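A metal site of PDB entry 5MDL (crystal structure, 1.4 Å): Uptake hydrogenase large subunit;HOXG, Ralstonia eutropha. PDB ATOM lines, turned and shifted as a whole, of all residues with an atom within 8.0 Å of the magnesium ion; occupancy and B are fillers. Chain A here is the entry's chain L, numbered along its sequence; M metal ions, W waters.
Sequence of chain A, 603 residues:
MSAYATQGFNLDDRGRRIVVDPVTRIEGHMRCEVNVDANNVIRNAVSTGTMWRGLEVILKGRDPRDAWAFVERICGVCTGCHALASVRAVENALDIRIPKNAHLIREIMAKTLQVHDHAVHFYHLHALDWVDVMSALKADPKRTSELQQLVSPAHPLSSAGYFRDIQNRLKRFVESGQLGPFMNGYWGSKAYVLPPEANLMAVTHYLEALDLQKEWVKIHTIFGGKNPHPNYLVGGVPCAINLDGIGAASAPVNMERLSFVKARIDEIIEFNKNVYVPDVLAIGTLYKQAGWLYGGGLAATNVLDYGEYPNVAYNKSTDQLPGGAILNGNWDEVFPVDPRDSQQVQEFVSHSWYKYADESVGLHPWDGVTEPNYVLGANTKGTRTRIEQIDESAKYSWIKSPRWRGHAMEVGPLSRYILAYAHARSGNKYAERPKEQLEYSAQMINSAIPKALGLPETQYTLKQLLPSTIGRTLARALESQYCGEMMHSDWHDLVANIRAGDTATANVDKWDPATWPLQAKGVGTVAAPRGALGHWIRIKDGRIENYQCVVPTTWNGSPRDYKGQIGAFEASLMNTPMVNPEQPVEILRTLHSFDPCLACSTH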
ATOM      1  N   TRP A  52       8.796  15.121 -22.576  1.00  0.00           N
ATOM      2  CA  TRP A  52       8.188  13.879 -22.146  1.00  0.00           C
ATOM      3  C   TRP A  52       7.725  13.130 -23.370  1.00  0.00           C
ATOM      4  O   TRP A  52       7.317  13.744 -24.358  1.00  0.00           O
ATOM      5  CB  TRP A  52       7.012  14.132 -21.190  1.00  0.00           C
ATOM      6  CG  TRP A  52       6.302  12.883 -20.747  1.00  0.00           C
ATOM      7  CD1 TRP A  52       6.799  11.881 -19.969  1.00  0.00           C
ATOM      8  CD2 TRP A  52       4.939  12.533 -21.036  1.00  0.00           C
ATOM      9  NE1 TRP A  52       5.845  10.903 -19.786  1.00  0.00           N
ATOM     10  CE2 TRP A  52       4.691  11.290 -20.415  1.00  0.00           C
ATOM     11  CE3 TRP A  52       3.899  13.151 -21.759  1.00  0.00           C
ATOM     12  CZ2 TRP A  52       3.449  10.644 -20.509  1.00  0.00           C
ATOM     13  CZ3 TRP A  52       2.674  12.492 -21.858  1.00  0.00           C
ATOM     14  CH2 TRP A  52       2.453  11.256 -21.227  1.00  0.00           C
ATOM     15  N   GLU A  56       6.185   4.694 -20.451  1.00  0.00           N
ATOM     16  CA  GLU A  56       5.483   3.832 -19.505  1.00  0.00           C
ATOM     17  C   GLU A  56       4.064   3.526 -19.969  1.00  0.00           C
ATOM     18  O   GLU A  56       3.570   2.431 -19.771  1.00  0.00           O
ATOM     19  CB  GLU A  56       5.472   4.466 -18.110  1.00  0.00           C
ATOM     20  CG  GLU A  56       6.872   4.552 -17.489  1.00  0.00           C
ATOM     21  CD  GLU A  56       7.022   5.671 -16.474  1.00  0.00           C
ATOM     22  OE1 GLU A  56       6.344   6.711 -16.601  1.00  0.00           O
ATOM     23  OE2 GLU A  56       7.898   5.528 -15.586  1.00  0.00           O
ATOM     24  N   ILE A  74      14.588   4.811 -24.376  1.00  0.00           N
ATOM     25  CA  ILE A  74      14.550   5.937 -23.452  1.00  0.00           C
ATOM     26  C   ILE A  74      15.779   6.829 -23.685  1.00  0.00           C
ATOM     27  O   ILE A  74      15.691   8.065 -23.617  1.00  0.00           O
ATOM     28  CB  ILE A  74      14.458   5.479 -21.994  1.00  0.00           C
ATOM     29  CG1 ILE A  74      13.065   4.920 -21.724  1.00  0.00           C
ATOM     30  CG2 ILE A  74      14.810   6.611 -21.026  1.00  0.00           C
ATOM     31  CD1 ILE A  74      12.940   4.221 -20.378  1.00  0.00           C
ATOM     32  N   GLU A 347       7.559   7.995  -5.683  1.00  0.00           N
ATOM     33  CA  GLU A 347       7.585   9.189  -6.525  1.00  0.00           C
ATOM     34  C   GLU A 347       6.385  10.071  -6.265  1.00  0.00           C
ATOM     35  O   GLU A 347       5.238   9.606  -6.308  1.00  0.00           O
ATOM     36  CB  GLU A 347       7.628   8.828  -8.003  1.00  0.00           C
ATOM     37  CG  GLU A 347       8.925   8.150  -8.437  1.00  0.00           C
ATOM     38  CD  GLU A 347       8.891   7.803  -9.897  1.00  0.00           C
ATOM     39  OE1 GLU A 347       8.057   6.953 -10.271  1.00  0.00           O
ATOM     40  OE2 GLU A 347       9.701   8.394 -10.635  1.00  0.00           O
ATOM     41  N   TYR A 354       2.068  15.881 -13.923  1.00  0.00           N
ATOM     42  CA  TYR A 354       1.285  14.639 -13.876  1.00  0.00           C
ATOM     43  C   TYR A 354       0.197  14.795 -12.845  1.00  0.00           C
ATOM     44  O   TYR A 354       0.160  15.772 -12.078  1.00  0.00           O
ATOM     45  CB  TYR A 354       2.169  13.444 -13.507  1.00  0.00           C
ATOM     46  CG  TYR A 354       3.356  13.282 -14.415  1.00  0.00           C
ATOM     47  CD1 TYR A 354       3.215  12.704 -15.683  1.00  0.00           C
ATOM     48  CD2 TYR A 354       4.608  13.756 -14.044  1.00  0.00           C
ATOM     49  CE1 TYR A 354       4.312  12.594 -16.539  1.00  0.00           C
ATOM     50  CE2 TYR A 354       5.703  13.640 -14.892  1.00  0.00           C
ATOM     51  CZ  TYR A 354       5.547  13.075 -16.130  1.00  0.00           C
ATOM     52  OH  TYR A 354       6.615  12.965 -16.967  1.00  0.00           O
ATOM     53  N   PRO A 365       6.947   2.329  -7.308  1.00  0.00           N
ATOM     54  CA  PRO A 365       6.730   2.184  -8.758  1.00  0.00           C
ATOM     55  C   PRO A 365       5.871   0.979  -9.209  1.00  0.00           C
ATOM     56  O   PRO A 365       5.281   1.047 -10.270  1.00  0.00           O
ATOM     57  CB  PRO A 365       8.156   2.089  -9.322  1.00  0.00           C
ATOM     58  CG  PRO A 365       9.000   2.753  -8.282  1.00  0.00           C
ATOM     59  CD  PRO A 365       8.379   2.381  -6.980  1.00  0.00           C
ATOM     60  N   GLY A 368       2.849   2.756  -9.540  1.00  0.00           N
ATOM     61  CA  GLY A 368       3.030   4.059 -10.172  1.00  0.00           C
ATOM     62  C   GLY A 368       1.985   4.362 -11.231  1.00  0.00           C
ATOM     63  O   GLY A 368       1.370   3.451 -11.818  1.00  0.00           O
ATOM     64  N   VAL A 369       1.798   5.656 -11.471  1.00  0.00           N
ATOM     65  CA  VAL A 369       0.800   6.188 -12.386  1.00  0.00           C
ATOM     66  C   VAL A 369       1.455   7.299 -13.193  1.00  0.00           C
ATOM     67  O   VAL A 369       2.157   8.129 -12.629  1.00  0.00           O
ATOM     68  CB  VAL A 369      -0.410   6.770 -11.586  1.00  0.00           C
ATOM     69  CG1 VAL A 369      -1.401   7.449 -12.514  1.00  0.00           C
ATOM     70  CG2 VAL A 369      -1.075   5.670 -10.762  1.00  0.00           C
ATOM     71  N   THR A 370       1.259   7.288 -14.505  1.00  0.00           N
ATOM     72  CA  THR A 370       1.786   8.326 -15.385  1.00  0.00           C
ATOM     73  C   THR A 370       0.667   8.878 -16.262  1.00  0.00           C
ATOM     74  O   THR A 370       0.468   8.447 -17.399  1.00  0.00           O
ATOM     75  CB  THR A 370       2.944   7.795 -16.234  1.00  0.00           C
ATOM     76  OG1 THR A 370       3.889   7.165 -15.369  1.00  0.00           O
ATOM     77  CG2 THR A 370       3.603   8.912 -17.025  1.00  0.00           C
ATOM     78  N   TRP A 398       8.480  18.060 -16.236  1.00  0.00           N
ATOM     79  CA  TRP A 398       8.075  16.727 -16.680  1.00  0.00           C
ATOM     80  C   TRP A 398       8.762  15.608 -15.879  1.00  0.00           C
ATOM     81  O   TRP A 398       8.486  14.433 -16.112  1.00  0.00           O
ATOM     82  CB  TRP A 398       8.355  16.566 -18.176  1.00  0.00           C
ATOM     83  CG  TRP A 398       7.385  17.282 -19.039  1.00  0.00           C
ATOM     84  CD1 TRP A 398       7.620  18.377 -19.806  1.00  0.00           C
ATOM     85  CD2 TRP A 398       5.990  16.962 -19.206  1.00  0.00           C
ATOM     86  NE1 TRP A 398       6.455  18.761 -20.464  1.00  0.00           N
ATOM     87  CE2 TRP A 398       5.444  17.906 -20.104  1.00  0.00           C
ATOM     88  CE3 TRP A 398       5.159  15.961 -18.689  1.00  0.00           C
ATOM     89  CZ2 TRP A 398       4.095  17.880 -20.495  1.00  0.00           C
ATOM     90  CZ3 TRP A 398       3.823  15.929 -19.080  1.00  0.00           C
ATOM     91  CH2 TRP A 398       3.314  16.889 -19.973  1.00  0.00           C
ATOM     92  N   ILE A 399       9.648  15.951 -14.941  1.00  0.00           N
ATOM     93  CA  ILE A 399      10.329  14.955 -14.098  1.00  0.00           C
ATOM     94  C   ILE A 399       9.497  14.727 -12.841  1.00  0.00           C
ATOM     95  O   ILE A 399       9.121  15.701 -12.168  1.00  0.00           O
ATOM     96  CB  ILE A 399      11.759  15.410 -13.716  1.00  0.00           C
ATOM     97  CG1 ILE A 399      12.518  15.845 -14.963  1.00  0.00           C
ATOM     98  CG2 ILE A 399      12.493  14.288 -13.004  1.00  0.00           C
ATOM     99  CD1 ILE A 399      13.887  16.435 -14.723  1.00  0.00           C
ATOM    100  N   LYS A 400       9.218  13.463 -12.505  1.00  0.00           N
ATOM    101  CA  LYS A 400       8.646  13.114 -11.203  1.00  0.00           C
ATOM    102  C   LYS A 400       9.658  13.354 -10.053  1.00  0.00           C
ATOM    103  O   LYS A 400      10.832  13.611 -10.308  1.00  0.00           O
ATOM    104  CB  LYS A 400       8.168  11.655 -11.188  1.00  0.00           C
ATOM    105  CG  LYS A 400       7.031  11.342 -12.156  1.00  0.00           C
ATOM    106  CD  LYS A 400       6.485   9.937 -11.915  1.00  0.00           C
ATOM    107  CE  LYS A 400       5.356   9.564 -12.859  1.00  0.00           C
ATOM    108  NZ  LYS A 400       5.096   8.108 -12.836  1.00  0.00           N
ATOM    109  N   PRO A 402      11.343  11.455  -7.159  1.00  0.00           N
ATOM    110  CA  PRO A 402      11.622  10.276  -6.344  1.00  0.00           C
ATOM    111  C   PRO A 402      12.240  10.643  -5.009  1.00  0.00           C
ATOM    112  O   PRO A 402      13.079  11.539  -4.942  1.00  0.00           O
ATOM    113  CB  PRO A 402      12.619   9.475  -7.206  1.00  0.00           C
ATOM    114  CG  PRO A 402      12.630  10.141  -8.548  1.00  0.00           C
ATOM    115  CD  PRO A 402      12.316  11.566  -8.258  1.00  0.00           C
ATOM    116  N   GLY A 534      16.028   1.888 -11.784  1.00  0.00           N
ATOM    117  CA  GLY A 534      15.130   0.767 -11.585  1.00  0.00           C
ATOM    118  C   GLY A 534      13.975   0.743 -12.576  1.00  0.00           C
ATOM    119  O   GLY A 534      13.465   1.792 -12.977  1.00  0.00           O
ATOM    120  N   TRP A 536      10.255  -1.369 -12.800  1.00  0.00           N
ATOM    121  CA  TRP A 536       9.314  -2.180 -12.049  1.00  0.00           C
ATOM    122  C   TRP A 536       8.192  -2.593 -12.982  1.00  0.00           C
ATOM    123  O   TRP A 536       7.526  -1.734 -13.560  1.00  0.00           O
ATOM    124  CB  TRP A 536       8.733  -1.339 -10.910  1.00  0.00           C
ATOM    125  CG  TRP A 536       9.619  -1.151  -9.711  1.00  0.00           C
ATOM    126  CD1 TRP A 536       9.548  -1.821  -8.528  1.00  0.00           C
ATOM    127  CD2 TRP A 536      10.658  -0.175  -9.564  1.00  0.00           C
ATOM    128  NE1 TRP A 536      10.494  -1.342  -7.648  1.00  0.00           N
ATOM    129  CE2 TRP A 536      11.175  -0.317  -8.252  1.00  0.00           C
ATOM    130  CE3 TRP A 536      11.196   0.809 -10.404  1.00  0.00           C
ATOM    131  CZ2 TRP A 536      12.221   0.471  -7.779  1.00  0.00           C
ATOM    132  CZ3 TRP A 536      12.233   1.608  -9.914  1.00  0.00           C
ATOM    133  CH2 TRP A 536      12.720   1.434  -8.616  1.00  0.00           C
ATOM    134  N   TYR A 547       4.308  -0.734 -16.118  1.00  0.00           N
ATOM    135  CA  TYR A 547       5.740  -0.665 -16.298  1.00  0.00           C
ATOM    136  C   TYR A 547       6.162   0.748 -15.871  1.00  0.00           C
ATOM    137  O   TYR A 547       5.788   1.727 -16.520  1.00  0.00           O
ATOM    138  CB  TYR A 547       6.130  -0.934 -17.769  1.00  0.00           C
ATOM    139  CG  TYR A 547       7.568  -1.362 -17.943  1.00  0.00           C
ATOM    140  CD1 TYR A 547       8.624  -0.496 -17.671  1.00  0.00           C
ATOM    141  CD2 TYR A 547       7.886  -2.667 -18.335  1.00  0.00           C
ATOM    142  CE1 TYR A 547       9.944  -0.899 -17.815  1.00  0.00           C
ATOM    143  CE2 TYR A 547       9.191  -3.070 -18.470  1.00  0.00           C
ATOM    144  CZ  TYR A 547      10.222  -2.192 -18.196  1.00  0.00           C
ATOM    145  OH  TYR A 547      11.522  -2.606 -18.339  1.00  0.00           O
ATOM    146  N   GLN A 548       6.935   0.836 -14.795  1.00  0.00           N
ATOM    147  CA  GLN A 548       7.347   2.132 -14.253  1.00  0.00           C
ATOM    148  C   GLN A 548       8.862   2.180 -14.140  1.00  0.00           C
ATOM    149  O   GLN A 548       9.502   1.255 -13.621  1.00  0.00           O
ATOM    150  CB  GLN A 548       6.701   2.399 -12.894  1.00  0.00           C
ATOM    151  CG  GLN A 548       5.195   2.655 -12.965  1.00  0.00           C
ATOM    152  CD  GLN A 548       4.835   4.004 -13.577  1.00  0.00           C
ATOM    153  OE1 GLN A 548       5.497   5.017 -13.337  1.00  0.00           O
ATOM    154  NE2 GLN A 548       3.789   4.021 -14.363  1.00  0.00           N
ATOM    155  N   CYS A 549       9.430   3.268 -14.642  1.00  0.00           N
ATOM    156  CA  CYS A 549      10.856   3.497 -14.575  1.00  0.00           C
ATOM    157  C   CYS A 549      11.134   4.660 -13.639  1.00  0.00           C
ATOM    158  O   CYS A 549      10.457   5.713 -13.721  1.00  0.00           O
ATOM    159  CB  CYS A 549      11.388   3.854 -15.952  1.00  0.00           C
ATOM    160  SG  CYS A 549      11.053   2.642 -17.257  1.00  0.00           S
ATOM    161  N   VAL A 550      12.130   4.478 -12.776  1.00  0.00           N
ATOM    162  CA  VAL A 550      12.678   5.574 -11.974  1.00  0.00           C
ATOM    163  C   VAL A 550      14.167   5.583 -12.290  1.00  0.00           C
ATOM    164  O   VAL A 550      14.880   4.620 -12.022  1.00  0.00           O
ATOM    165  CB  VAL A 550      12.443   5.384 -10.455  1.00  0.00           C
ATOM    166  CG1 VAL A 550      12.839   6.660  -9.711  1.00  0.00           C
ATOM    167  CG2 VAL A 550      10.999   5.010 -10.160  1.00  0.00           C
ATOM    168  N   VAL A 551      14.628   6.688 -12.874  1.00  0.00           N
ATOM    169  CA  VAL A 551      15.880   6.742 -13.618  1.00  0.00           C
ATOM    170  C   VAL A 551      16.819   7.715 -12.854  1.00  0.00           C
ATOM    171  O   VAL A 551      16.335   8.543 -12.079  1.00  0.00           O
ATOM    172  CB  VAL A 551      15.552   7.139 -15.090  1.00  0.00           C
ATOM    173  CG1 VAL A 551      16.735   7.078 -16.006  1.00  0.00           C
ATOM    174  CG2 VAL A 551      14.462   6.228 -15.651  1.00  0.00           C
ATOM    175  N   THR A 554      16.024  11.242 -12.981  1.00  0.00           N
ATOM    176  CA  THR A 554      14.759  11.494 -12.284  1.00  0.00           C
ATOM    177  C   THR A 554      15.034  11.883 -10.822  1.00  0.00           C
ATOM    178  O   THR A 554      14.496  12.888 -10.329  1.00  0.00           O
ATOM    179  CB  THR A 554      13.793  10.289 -12.310  1.00  0.00           C
ATOM    180  OG1 THR A 554      13.767   9.680 -13.624  1.00  0.00           O
ATOM    181  CG2 THR A 554      12.386  10.735 -11.938  1.00  0.00           C
ATOM    182  N   CYS A 600      16.236  10.399 -20.319  1.00  0.00           N
ATOM    183  CA  CYS A 600      16.185   9.430 -19.229  1.00  0.00           C
ATOM    184  C   CYS A 600      15.261   9.864 -18.107  1.00  0.00           C
ATOM    185  O   CYS A 600      14.469   9.083 -17.596  1.00  0.00           O
ATOM    186  CB  CYS A 600      17.577   9.230 -18.637  1.00  0.00           C
ATOM    187  SG  CYS A 600      18.425   7.808 -19.314  1.00  0.00           S
ATOM    188  N   SER A 601      15.391  11.117 -17.695  1.00  0.00           N
ATOM    189  CA  SER A 601      14.723  11.577 -16.482  1.00  0.00           C
ATOM    190  C   SER A 601      13.213  11.521 -16.599  1.00  0.00           C
ATOM    191  O   SER A 601      12.536  11.289 -15.603  1.00  0.00           O
ATOM    192  CB  SER A 601      15.160  13.001 -16.129  1.00  0.00           C
ATOM    193  OG  SER A 601      14.616  13.996 -16.983  1.00  0.00           O
ATOM    194  N   THR A 602      12.719  11.700 -17.822  1.00  0.00           N
ATOM    195  CA  THR A 602      11.288  11.862 -18.108  1.00  0.00           C
ATOM    196  C   THR A 602      10.669  10.630 -18.794  1.00  0.00           C
ATOM    197  O   THR A 602       9.518  10.283 -18.534  1.00  0.00           O
ATOM    198  CB  THR A 602      11.076  13.104 -19.002  1.00  0.00           C
ATOM    199  OG1 THR A 602      11.891  13.021 -20.185  1.00  0.00           O
ATOM    200  CG2 THR A 602      11.446  14.367 -18.236  1.00  0.00           C
ATOM    201  N   HIS A 603      11.433   9.995 -19.692  1.00  0.00           N
ATOM    202  CA  HIS A 603      10.981   8.780 -20.395  1.00  0.00           C
ATOM    203  C   HIS A 603       9.531   8.876 -20.872  1.00  0.00           C
ATOM    204  O   HIS A 603       8.702   7.963 -20.719  1.00  0.00           O
ATOM    205  CB  HIS A 603      11.298   7.497 -19.604  1.00  0.00           C
ATOM    206  CG  HIS A 603      11.008   7.586 -18.145  1.00  0.00           C
ATOM    207  ND1 HIS A 603      11.871   8.175 -17.245  1.00  0.00           N
ATOM    208  CD2 HIS A 603       9.949   7.156 -17.424  1.00  0.00           C
ATOM    209  CE1 HIS A 603      11.339   8.121 -16.035  1.00  0.00           C
ATOM    210  NE2 HIS A 603      10.177   7.498 -16.122  1.00  0.00           N
ATOM    211  OXT HIS A 603       9.194   9.897 -21.475  1.00  0.00           O
HETATM  212 MG    MG M   1       8.889   6.976 -14.349  1.00  0.00          MG
HETATM  213  O   HOH W   1       7.723   6.382 -12.815  1.00  0.00           O
HETATM  214  O   HOH W   2       7.457   8.408 -14.939  1.00  0.00           O
HETATM  215  O   HOH W   3       9.824   8.494 -13.223  1.00  0.00           O
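The magnesium ion is bound by water W1 (2.0 Å), water W3 (2.1 Å), water W2 (2.1 Å), O of Cys 549 (2.1 Å), OE2 of Glu 56 (2.1 Å) and NE2 of His 603 (2.3 Å).
Water W2 bridges OE1 of Glu 56 (2.6 Å) and NZ of Lys 400 (3.2 Å).
Water W1 lies within hydrogen-bond range of the side-chain carboxylate (OE1) of Glu 347 (2.6 Å), the side-chain amide oxygen (OE1) of Gln 548 (2.7 Å) and the side-chain amino group (NZ) of Lys 400 (3.1 Å).
Within 4 Å of the magnesium ion: Glu 56, Cys 549 and His 603.
The nearest printed residue that does not touch the magnesium ion is Gln 548 (4.05 Å).
OE2 of Glu 56 sits close to OE1 of Gln 548 (3.3 Å).
The side-chain carboxylate (OE1) of Glu 56 is in hydrogen-bond range of the side-chain hydroxyl (OG1) of Thr 370 (2.8 Å).
The backbone carbonyl oxygen (O) of Cys 600 lies within hydrogen-bond range of a ring nitrogen (ND1) of His 603 (2.8 Å).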
